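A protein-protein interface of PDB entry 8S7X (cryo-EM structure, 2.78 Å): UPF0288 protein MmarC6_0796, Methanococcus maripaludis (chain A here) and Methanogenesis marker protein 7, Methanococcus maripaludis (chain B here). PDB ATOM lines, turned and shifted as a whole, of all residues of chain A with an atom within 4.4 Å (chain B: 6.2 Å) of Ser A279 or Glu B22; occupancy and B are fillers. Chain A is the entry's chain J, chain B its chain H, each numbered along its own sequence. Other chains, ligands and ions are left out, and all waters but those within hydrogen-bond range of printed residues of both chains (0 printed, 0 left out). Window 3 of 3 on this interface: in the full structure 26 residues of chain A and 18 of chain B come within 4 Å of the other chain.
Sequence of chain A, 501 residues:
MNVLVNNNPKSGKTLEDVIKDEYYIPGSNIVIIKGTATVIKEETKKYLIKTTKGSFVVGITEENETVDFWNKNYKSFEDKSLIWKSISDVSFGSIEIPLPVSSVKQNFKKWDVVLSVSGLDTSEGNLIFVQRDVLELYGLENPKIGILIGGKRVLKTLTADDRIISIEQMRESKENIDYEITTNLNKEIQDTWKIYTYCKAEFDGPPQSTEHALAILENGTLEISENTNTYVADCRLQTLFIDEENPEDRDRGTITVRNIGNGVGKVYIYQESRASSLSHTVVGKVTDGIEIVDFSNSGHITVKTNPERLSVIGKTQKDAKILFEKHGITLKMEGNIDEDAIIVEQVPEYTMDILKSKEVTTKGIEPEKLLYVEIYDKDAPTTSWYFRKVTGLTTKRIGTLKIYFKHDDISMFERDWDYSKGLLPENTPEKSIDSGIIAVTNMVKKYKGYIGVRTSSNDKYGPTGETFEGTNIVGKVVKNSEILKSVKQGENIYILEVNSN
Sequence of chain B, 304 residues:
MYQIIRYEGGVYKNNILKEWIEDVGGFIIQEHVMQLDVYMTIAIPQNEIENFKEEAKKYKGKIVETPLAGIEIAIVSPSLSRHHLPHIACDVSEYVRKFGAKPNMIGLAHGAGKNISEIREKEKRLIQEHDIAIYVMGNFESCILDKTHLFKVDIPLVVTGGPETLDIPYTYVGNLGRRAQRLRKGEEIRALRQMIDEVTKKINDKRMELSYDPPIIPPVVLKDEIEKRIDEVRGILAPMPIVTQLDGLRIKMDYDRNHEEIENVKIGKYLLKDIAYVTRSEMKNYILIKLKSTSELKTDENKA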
ATOM      1  N   ARG A 250      15.723  -3.857  -7.903  1.00  0.00           N
ATOM      2  CA  ARG A 250      15.353  -4.486  -9.169  1.00  0.00           C
ATOM      3  C   ARG A 250      16.233  -3.885 -10.258  1.00  0.00           C
ATOM      4  O   ARG A 250      15.827  -3.016 -11.030  1.00  0.00           O
ATOM      5  CB  ARG A 250      13.872  -4.288  -9.454  1.00  0.00           C
ATOM      6  CG  ARG A 250      12.965  -4.880  -8.397  1.00  0.00           C
ATOM      7  CD  ARG A 250      11.514  -4.541  -8.662  1.00  0.00           C
ATOM      8  NE  ARG A 250      11.191  -3.176  -8.266  1.00  0.00           N
ATOM      9  CZ  ARG A 250      10.035  -2.579  -8.520  1.00  0.00           C
ATOM     10  NH1 ARG A 250       9.072  -3.197  -9.180  1.00  0.00           N
ATOM     11  NH2 ARG A 250       9.843  -1.334  -8.103  1.00  0.00           N
ATOM     12  N   VAL A 257       9.546 -12.352  -8.678  1.00  0.00           N
ATOM     13  CA  VAL A 257       8.229 -12.968  -8.643  1.00  0.00           C
ATOM     14  C   VAL A 257       7.350 -12.113  -7.745  1.00  0.00           C
ATOM     15  O   VAL A 257       7.684 -11.894  -6.575  1.00  0.00           O
ATOM     16  CB  VAL A 257       8.283 -14.416  -8.132  1.00  0.00           C
ATOM     17  CG1 VAL A 257       6.909 -15.042  -8.195  1.00  0.00           C
ATOM     18  CG2 VAL A 257       9.267 -15.224  -8.946  1.00  0.00           C
ATOM     19  N   ARG A 258       6.238 -11.633  -8.286  1.00  0.00           N
ATOM     20  CA  ARG A 258       5.304 -10.860  -7.481  1.00  0.00           C
ATOM     21  C   ARG A 258       4.589 -11.781  -6.503  1.00  0.00           C
ATOM     22  O   ARG A 258       4.055 -12.821  -6.894  1.00  0.00           O
ATOM     23  CB  ARG A 258       4.297 -10.145  -8.375  1.00  0.00           C
ATOM     24  CG  ARG A 258       3.251  -9.363  -7.621  1.00  0.00           C
ATOM     25  CD  ARG A 258       2.424  -8.515  -8.560  1.00  0.00           C
ATOM     26  NE  ARG A 258       2.829  -7.119  -8.518  1.00  0.00           N
ATOM     27  CZ  ARG A 258       2.443  -6.261  -7.586  1.00  0.00           C
ATOM     28  NH1 ARG A 258       1.644  -6.627  -6.600  1.00  0.00           N
ATOM     29  NH2 ARG A 258       2.874  -5.005  -7.642  1.00  0.00           N
ATOM     30  N   ASN A 259       4.581 -11.402  -5.229  1.00  0.00           N
ATOM     31  CA  ASN A 259       4.126 -12.293  -4.174  1.00  0.00           C
ATOM     32  C   ASN A 259       2.811 -11.873  -3.536  1.00  0.00           C
ATOM     33  O   ASN A 259       2.382 -12.505  -2.566  1.00  0.00           O
ATOM     34  CB  ASN A 259       5.201 -12.407  -3.087  1.00  0.00           C
ATOM     35  CG  ASN A 259       5.622 -11.064  -2.544  1.00  0.00           C
ATOM     36  OD1 ASN A 259       5.079 -10.032  -2.923  1.00  0.00           O
ATOM     37  ND2 ASN A 259       6.599 -11.070  -1.653  1.00  0.00           N
ATOM     38  N   ILE A 260       2.151 -10.832  -4.045  1.00  0.00           N
ATOM     39  CA  ILE A 260       0.927 -10.338  -3.429  1.00  0.00           C
ATOM     40  C   ILE A 260       0.134  -9.591  -4.483  1.00  0.00           C
ATOM     41  O   ILE A 260       0.700  -9.032  -5.426  1.00  0.00           O
ATOM     42  CB  ILE A 260       1.241  -9.446  -2.202  1.00  0.00           C
ATOM     43  CG1 ILE A 260      -0.012  -9.239  -1.353  1.00  0.00           C
ATOM     44  CG2 ILE A 260       1.816  -8.113  -2.636  1.00  0.00           C
ATOM     45  CD1 ILE A 260      -0.503 -10.501  -0.675  1.00  0.00           C
ATOM     46  N   SER A 277      11.135  -3.211  -4.113  1.00  0.00           N
ATOM     47  CA  SER A 277       9.697  -3.272  -3.893  1.00  0.00           C
ATOM     48  C   SER A 277       9.378  -4.392  -2.917  1.00  0.00           C
ATOM     49  O   SER A 277       9.970  -5.471  -2.980  1.00  0.00           O
ATOM     50  CB  SER A 277       8.943  -3.493  -5.205  1.00  0.00           C
ATOM     51  OG  SER A 277       7.552  -3.606  -4.976  1.00  0.00           O
ATOM     52  N   LEU A 278       8.434  -4.128  -2.011  1.00  0.00           N
ATOM     53  CA  LEU A 278       8.014  -5.152  -1.064  1.00  0.00           C
ATOM     54  C   LEU A 278       7.139  -6.214  -1.711  1.00  0.00           C
ATOM     55  O   LEU A 278       7.002  -7.308  -1.155  1.00  0.00           O
ATOM     56  CB  LEU A 278       7.268  -4.512   0.106  1.00  0.00           C
ATOM     57  CG  LEU A 278       8.042  -4.363   1.418  1.00  0.00           C
ATOM     58  CD1 LEU A 278       8.216  -5.714   2.089  1.00  0.00           C
ATOM     59  CD2 LEU A 278       9.387  -3.700   1.181  1.00  0.00           C
ATOM     60  N   SER A 279       6.547  -5.920  -2.864  1.00  0.00           N
ATOM     61  CA  SER A 279       5.669  -6.855  -3.552  1.00  0.00           C
ATOM     62  C   SER A 279       6.394  -7.709  -4.576  1.00  0.00           C
ATOM     63  O   SER A 279       5.750  -8.507  -5.260  1.00  0.00           O
ATOM     64  CB  SER A 279       4.531  -6.101  -4.241  1.00  0.00           C
ATOM     65  OG  SER A 279       4.039  -5.062  -3.419  1.00  0.00           O
ATOM     66  N   HIS A 280       7.707  -7.559  -4.711  1.00  0.00           N
ATOM     67  CA  HIS A 280       8.490  -8.322  -5.671  1.00  0.00           C
ATOM     68  C   HIS A 280       9.568  -9.103  -4.938  1.00  0.00           C
ATOM     69  O   HIS A 280      10.361  -8.525  -4.190  1.00  0.00           O
ATOM     70  CB  HIS A 280       9.116  -7.404  -6.720  1.00  0.00           C
ATOM     71  CG  HIS A 280       8.136  -6.886  -7.722  1.00  0.00           C
ATOM     72  ND1 HIS A 280       7.972  -7.455  -8.965  1.00  0.00           N
ATOM     73  CD2 HIS A 280       7.260  -5.856  -7.660  1.00  0.00           C
ATOM     74  CE1 HIS A 280       7.040  -6.795  -9.629  1.00  0.00           C
ATOM     75  NE2 HIS A 280       6.592  -5.820  -8.860  1.00  0.00           N
ATOM     76  N   THR A 281       9.593 -10.413  -5.159  1.00  0.00           N
ATOM     77  CA  THR A 281      10.591 -11.296  -4.573  1.00  0.00           C
ATOM     78  C   THR A 281      11.611 -11.638  -5.649  1.00  0.00           C
ATOM     79  O   THR A 281      11.302 -12.372  -6.592  1.00  0.00           O
ATOM     80  CB  THR A 281       9.938 -12.563  -4.022  1.00  0.00           C
ATOM     81  OG1 THR A 281       8.868 -12.207  -3.141  1.00  0.00           O
ATOM     82  CG2 THR A 281      10.950 -13.397  -3.265  1.00  0.00           C
ATOM     83  N   LEU B  17      -4.349  -0.792 -10.548  1.00  0.00           N
ATOM     84  CA  LEU B  17      -3.539   0.289 -11.101  1.00  0.00           C
ATOM     85  C   LEU B  17      -2.351   0.603 -10.200  1.00  0.00           C
ATOM     86  O   LEU B  17      -1.247   0.869 -10.688  1.00  0.00           O
ATOM     87  CB  LEU B  17      -4.396   1.535 -11.308  1.00  0.00           C
ATOM     88  CG  LEU B  17      -3.668   2.737 -11.907  1.00  0.00           C
ATOM     89  CD1 LEU B  17      -3.493   2.566 -13.401  1.00  0.00           C
ATOM     90  CD2 LEU B  17      -4.412   4.015 -11.600  1.00  0.00           C
ATOM     91  N   LYS B  18      -2.560   0.586  -8.882  1.00  0.00           N
ATOM     92  CA  LYS B  18      -1.446   0.795  -7.964  1.00  0.00           C
ATOM     93  C   LYS B  18      -0.413  -0.316  -8.094  1.00  0.00           C
ATOM     94  O   LYS B  18       0.794  -0.067  -8.005  1.00  0.00           O
ATOM     95  CB  LYS B  18      -1.961   0.891  -6.531  1.00  0.00           C
ATOM     96  CG  LYS B  18      -2.781   2.131  -6.262  1.00  0.00           C
ATOM     97  CD  LYS B  18      -2.293   2.854  -5.028  1.00  0.00           C
ATOM     98  CE  LYS B  18      -2.883   2.253  -3.775  1.00  0.00           C
ATOM     99  NZ  LYS B  18      -4.267   2.731  -3.556  1.00  0.00           N
ATOM    100  N   GLU B  19      -0.872  -1.550  -8.305  1.00  0.00           N
ATOM    101  CA  GLU B  19       0.052  -2.653  -8.546  1.00  0.00           C
ATOM    102  C   GLU B  19       0.854  -2.429  -9.818  1.00  0.00           C
ATOM    103  O   GLU B  19       2.055  -2.710  -9.861  1.00  0.00           O
ATOM    104  CB  GLU B  19      -0.713  -3.969  -8.627  1.00  0.00           C
ATOM    105  CG  GLU B  19      -1.159  -4.508  -7.289  1.00  0.00           C
ATOM    106  CD  GLU B  19      -1.904  -5.813  -7.423  1.00  0.00           C
ATOM    107  OE1 GLU B  19      -1.608  -6.567  -8.372  1.00  0.00           O
ATOM    108  OE2 GLU B  19      -2.788  -6.085  -6.586  1.00  0.00           O
ATOM    109  N   TRP B  20       0.201  -1.942 -10.873  1.00  0.00           N
ATOM    110  CA  TRP B  20       0.913  -1.641 -12.113  1.00  0.00           C
ATOM    111  C   TRP B  20       1.967  -0.563 -11.891  1.00  0.00           C
ATOM    112  O   TRP B  20       3.092  -0.662 -12.402  1.00  0.00           O
ATOM    113  CB  TRP B  20      -0.077  -1.207 -13.189  1.00  0.00           C
ATOM    114  CG  TRP B  20       0.526  -1.012 -14.540  1.00  0.00           C
ATOM    115  CD1 TRP B  20       0.581  -1.925 -15.550  1.00  0.00           C
ATOM    116  CD2 TRP B  20       1.148   0.176 -15.040  1.00  0.00           C
ATOM    117  NE1 TRP B  20       1.204  -1.384 -16.643  1.00  0.00           N
ATOM    118  CE2 TRP B  20       1.561  -0.094 -16.355  1.00  0.00           C
ATOM    119  CE3 TRP B  20       1.395   1.441 -14.502  1.00  0.00           C
ATOM    120  CZ2 TRP B  20       2.211   0.853 -17.140  1.00  0.00           C
ATOM    121  CZ3 TRP B  20       2.041   2.377 -15.280  1.00  0.00           C
ATOM    122  CH2 TRP B  20       2.443   2.079 -16.585  1.00  0.00           C
ATOM    123  N   ILE B  21       1.616   0.474 -11.133  1.00  0.00           N
ATOM    124  CA  ILE B  21       2.562   1.550 -10.848  1.00  0.00           C
ATOM    125  C   ILE B  21       3.753   1.022 -10.062  1.00  0.00           C
ATOM    126  O   ILE B  21       4.905   1.391 -10.326  1.00  0.00           O
ATOM    127  CB  ILE B  21       1.853   2.700 -10.107  1.00  0.00           C
ATOM    128  CG1 ILE B  21       0.897   3.425 -11.045  1.00  0.00           C
ATOM    129  CG2 ILE B  21       2.862   3.668  -9.541  1.00  0.00           C
ATOM    130  CD1 ILE B  21      -0.162   4.219 -10.330  1.00  0.00           C
ATOM    131  N   GLU B  22       3.502   0.154  -9.079  1.00  0.00           N
ATOM    132  CA  GLU B  22       4.598  -0.474  -8.346  1.00  0.00           C
ATOM    133  C   GLU B  22       5.453  -1.336  -9.265  1.00  0.00           C
ATOM    134  O   GLU B  22       6.682  -1.364  -9.135  1.00  0.00           O
ATOM    135  CB  GLU B  22       4.054  -1.321  -7.197  1.00  0.00           C
ATOM    136  CG  GLU B  22       3.479  -0.530  -6.045  1.00  0.00           C
ATOM    137  CD  GLU B  22       2.624  -1.383  -5.128  1.00  0.00           C
ATOM    138  OE1 GLU B  22       2.684  -2.625  -5.244  1.00  0.00           O
ATOM    139  OE2 GLU B  22       1.890  -0.813  -4.293  1.00  0.00           O
ATOM    140  N   ASP B  23       4.817  -2.060 -10.185  1.00  0.00           N
ATOM    141  CA  ASP B  23       5.555  -2.933 -11.089  1.00  0.00           C
ATOM    142  C   ASP B  23       6.502  -2.139 -11.977  1.00  0.00           C
ATOM    143  O   ASP B  23       7.665  -2.518 -12.151  1.00  0.00           O
ATOM    144  CB  ASP B  23       4.587  -3.750 -11.940  1.00  0.00           C
ATOM    145  CG  ASP B  23       3.908  -4.851 -11.159  1.00  0.00           C
ATOM    146  OD1 ASP B  23       4.311  -5.093 -10.004  1.00  0.00           O
ATOM    147  OD2 ASP B  23       2.974  -5.478 -11.697  1.00  0.00           O
ATOM    148  N   VAL B  24       6.024  -1.030 -12.550  1.00  0.00           N
ATOM    149  CA  VAL B  24       6.878  -0.240 -13.437  1.00  0.00           C
ATOM    150  C   VAL B  24       7.828   0.671 -12.681  1.00  0.00           C
ATOM    151  O   VAL B  24       8.631   1.364 -13.314  1.00  0.00           O
ATOM    152  CB  VAL B  24       6.056   0.611 -14.423  1.00  0.00           C
ATOM    153  CG1 VAL B  24       5.056  -0.255 -15.155  1.00  0.00           C
ATOM    154  CG2 VAL B  24       5.364   1.738 -13.697  1.00  0.00           C
ATOM    155  N   GLY B  25       7.765   0.694 -11.357  1.00  0.00           N
ATOM    156  CA  GLY B  25       8.719   1.442 -10.568  1.00  0.00           C
ATOM    157  C   GLY B  25       8.296   2.830 -10.152  1.00  0.00           C
ATOM    158  O   GLY B  25       9.140   3.595  -9.673  1.00  0.00           O
ATOM    159  N   GLY B  26       7.028   3.186 -10.315  1.00  0.00           N
ATOM    160  CA  GLY B  26       6.567   4.485  -9.874  1.00  0.00           C
ATOM    161  C   GLY B  26       6.329   4.544  -8.377  1.00  0.00           C
ATOM    162  O   GLY B  26       6.396   3.549  -7.661  1.00  0.00           O
ATOM    163  N   ILE B  28       3.611   6.381  -5.411  1.00  0.00           N
ATOM    164  CA  ILE B  28       2.366   7.086  -5.128  1.00  0.00           C
ATOM    165  C   ILE B  28       2.679   8.111  -4.044  1.00  0.00           C
ATOM    166  O   ILE B  28       2.787   7.778  -2.864  1.00  0.00           O
ATOM    167  CB  ILE B  28       1.251   6.128  -4.711  1.00  0.00           C
ATOM    168  CG1 ILE B  28       0.816   5.273  -5.901  1.00  0.00           C
ATOM    169  CG2 ILE B  28       0.059   6.899  -4.188  1.00  0.00           C
ATOM    170  CD1 ILE B  28       1.314   3.854  -5.848  1.00  0.00           C
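The guanidinium group (NH1) of Arg A258 sits at hydrogen-bond distance from the backbone carbonyl oxygen (O) of Ile A260 (2.8 Å).
OG of Ser A277 lies close to N of Ser A279 (3.3 Å).
OD1 of Asn A259 sits close to O of Ser A279.
The side-chain carboxylate (OD1) of Asp B23 lies within salt-bridge range of the guanidinium group (NH2) of Arg A258 (2.8 Å).
The guanidinium group of Arg A258 lies within salt-bridge range of the side-chain carboxylate of Glu B19, 3.7 Å away.
OD1 of Asp B23 is in hydrogen-bond range of NE2 of His A280 (2.7 Å).
The backbone carbonyl oxygen of Asp B23 lies within hydrogen-bond range of the guanidinium group of Arg A250.
The side-chain hydroxyl (OG) of Ser A279 sits at hydrogen-bond distance from the side-chain carboxylate (OE1) of Glu B22, at 3.3 Å.
NH2 of Arg A258 is in salt-bridge range of OE1 of Glu B22, 3.4 Å away.
O of Glu B22 lies within hydrogen-bond range of NH1 of Arg A250, 3.0 Å away.
Among the printed residues, merely in contact across the chains: Arg A250 with Gly B25 (3.9 Å).
Printed residues of chain B within 4 Å of Arg A258: Glu B19, Glu B22 and Asp B23.
Of the printed residues of chain B, His A280 touches Asp B23 (2.7 Å).
Of the printed residues of chain A, Glu B19 touches Arg A258 (3.3 Å).
Of chain A, only Arg A250, Arg A258 and Ser A279 come within 4 Å of Glu B22.
Of the printed residues of chain A, Asp B23 touches Arg A250, Arg A258 and His A280.
Printed residues of chain A within 4 Å of Gly B25: Arg A250.
Ile B28 touches none of the printed residues of chain A.
The nearest residue of chain B that does not touch Ser A279 is Asp B23 (5.9 Å).
The nearest printed residue of chain A that does not touch Glu B22 is His A280 (4.5 Å).
The nearest printed residue of chain B that does not touch His A280 is Glu B22 (4.5 Å).
Of the 11 printed residues of chain B, 4 touch a printed residue of chain A.
Hydrophobic or aromatic side chains of chain A that line the printed part of chain B: His A280.
Along chain A the printed residues that touch a printed residue of chain B span positions 250 to 280.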
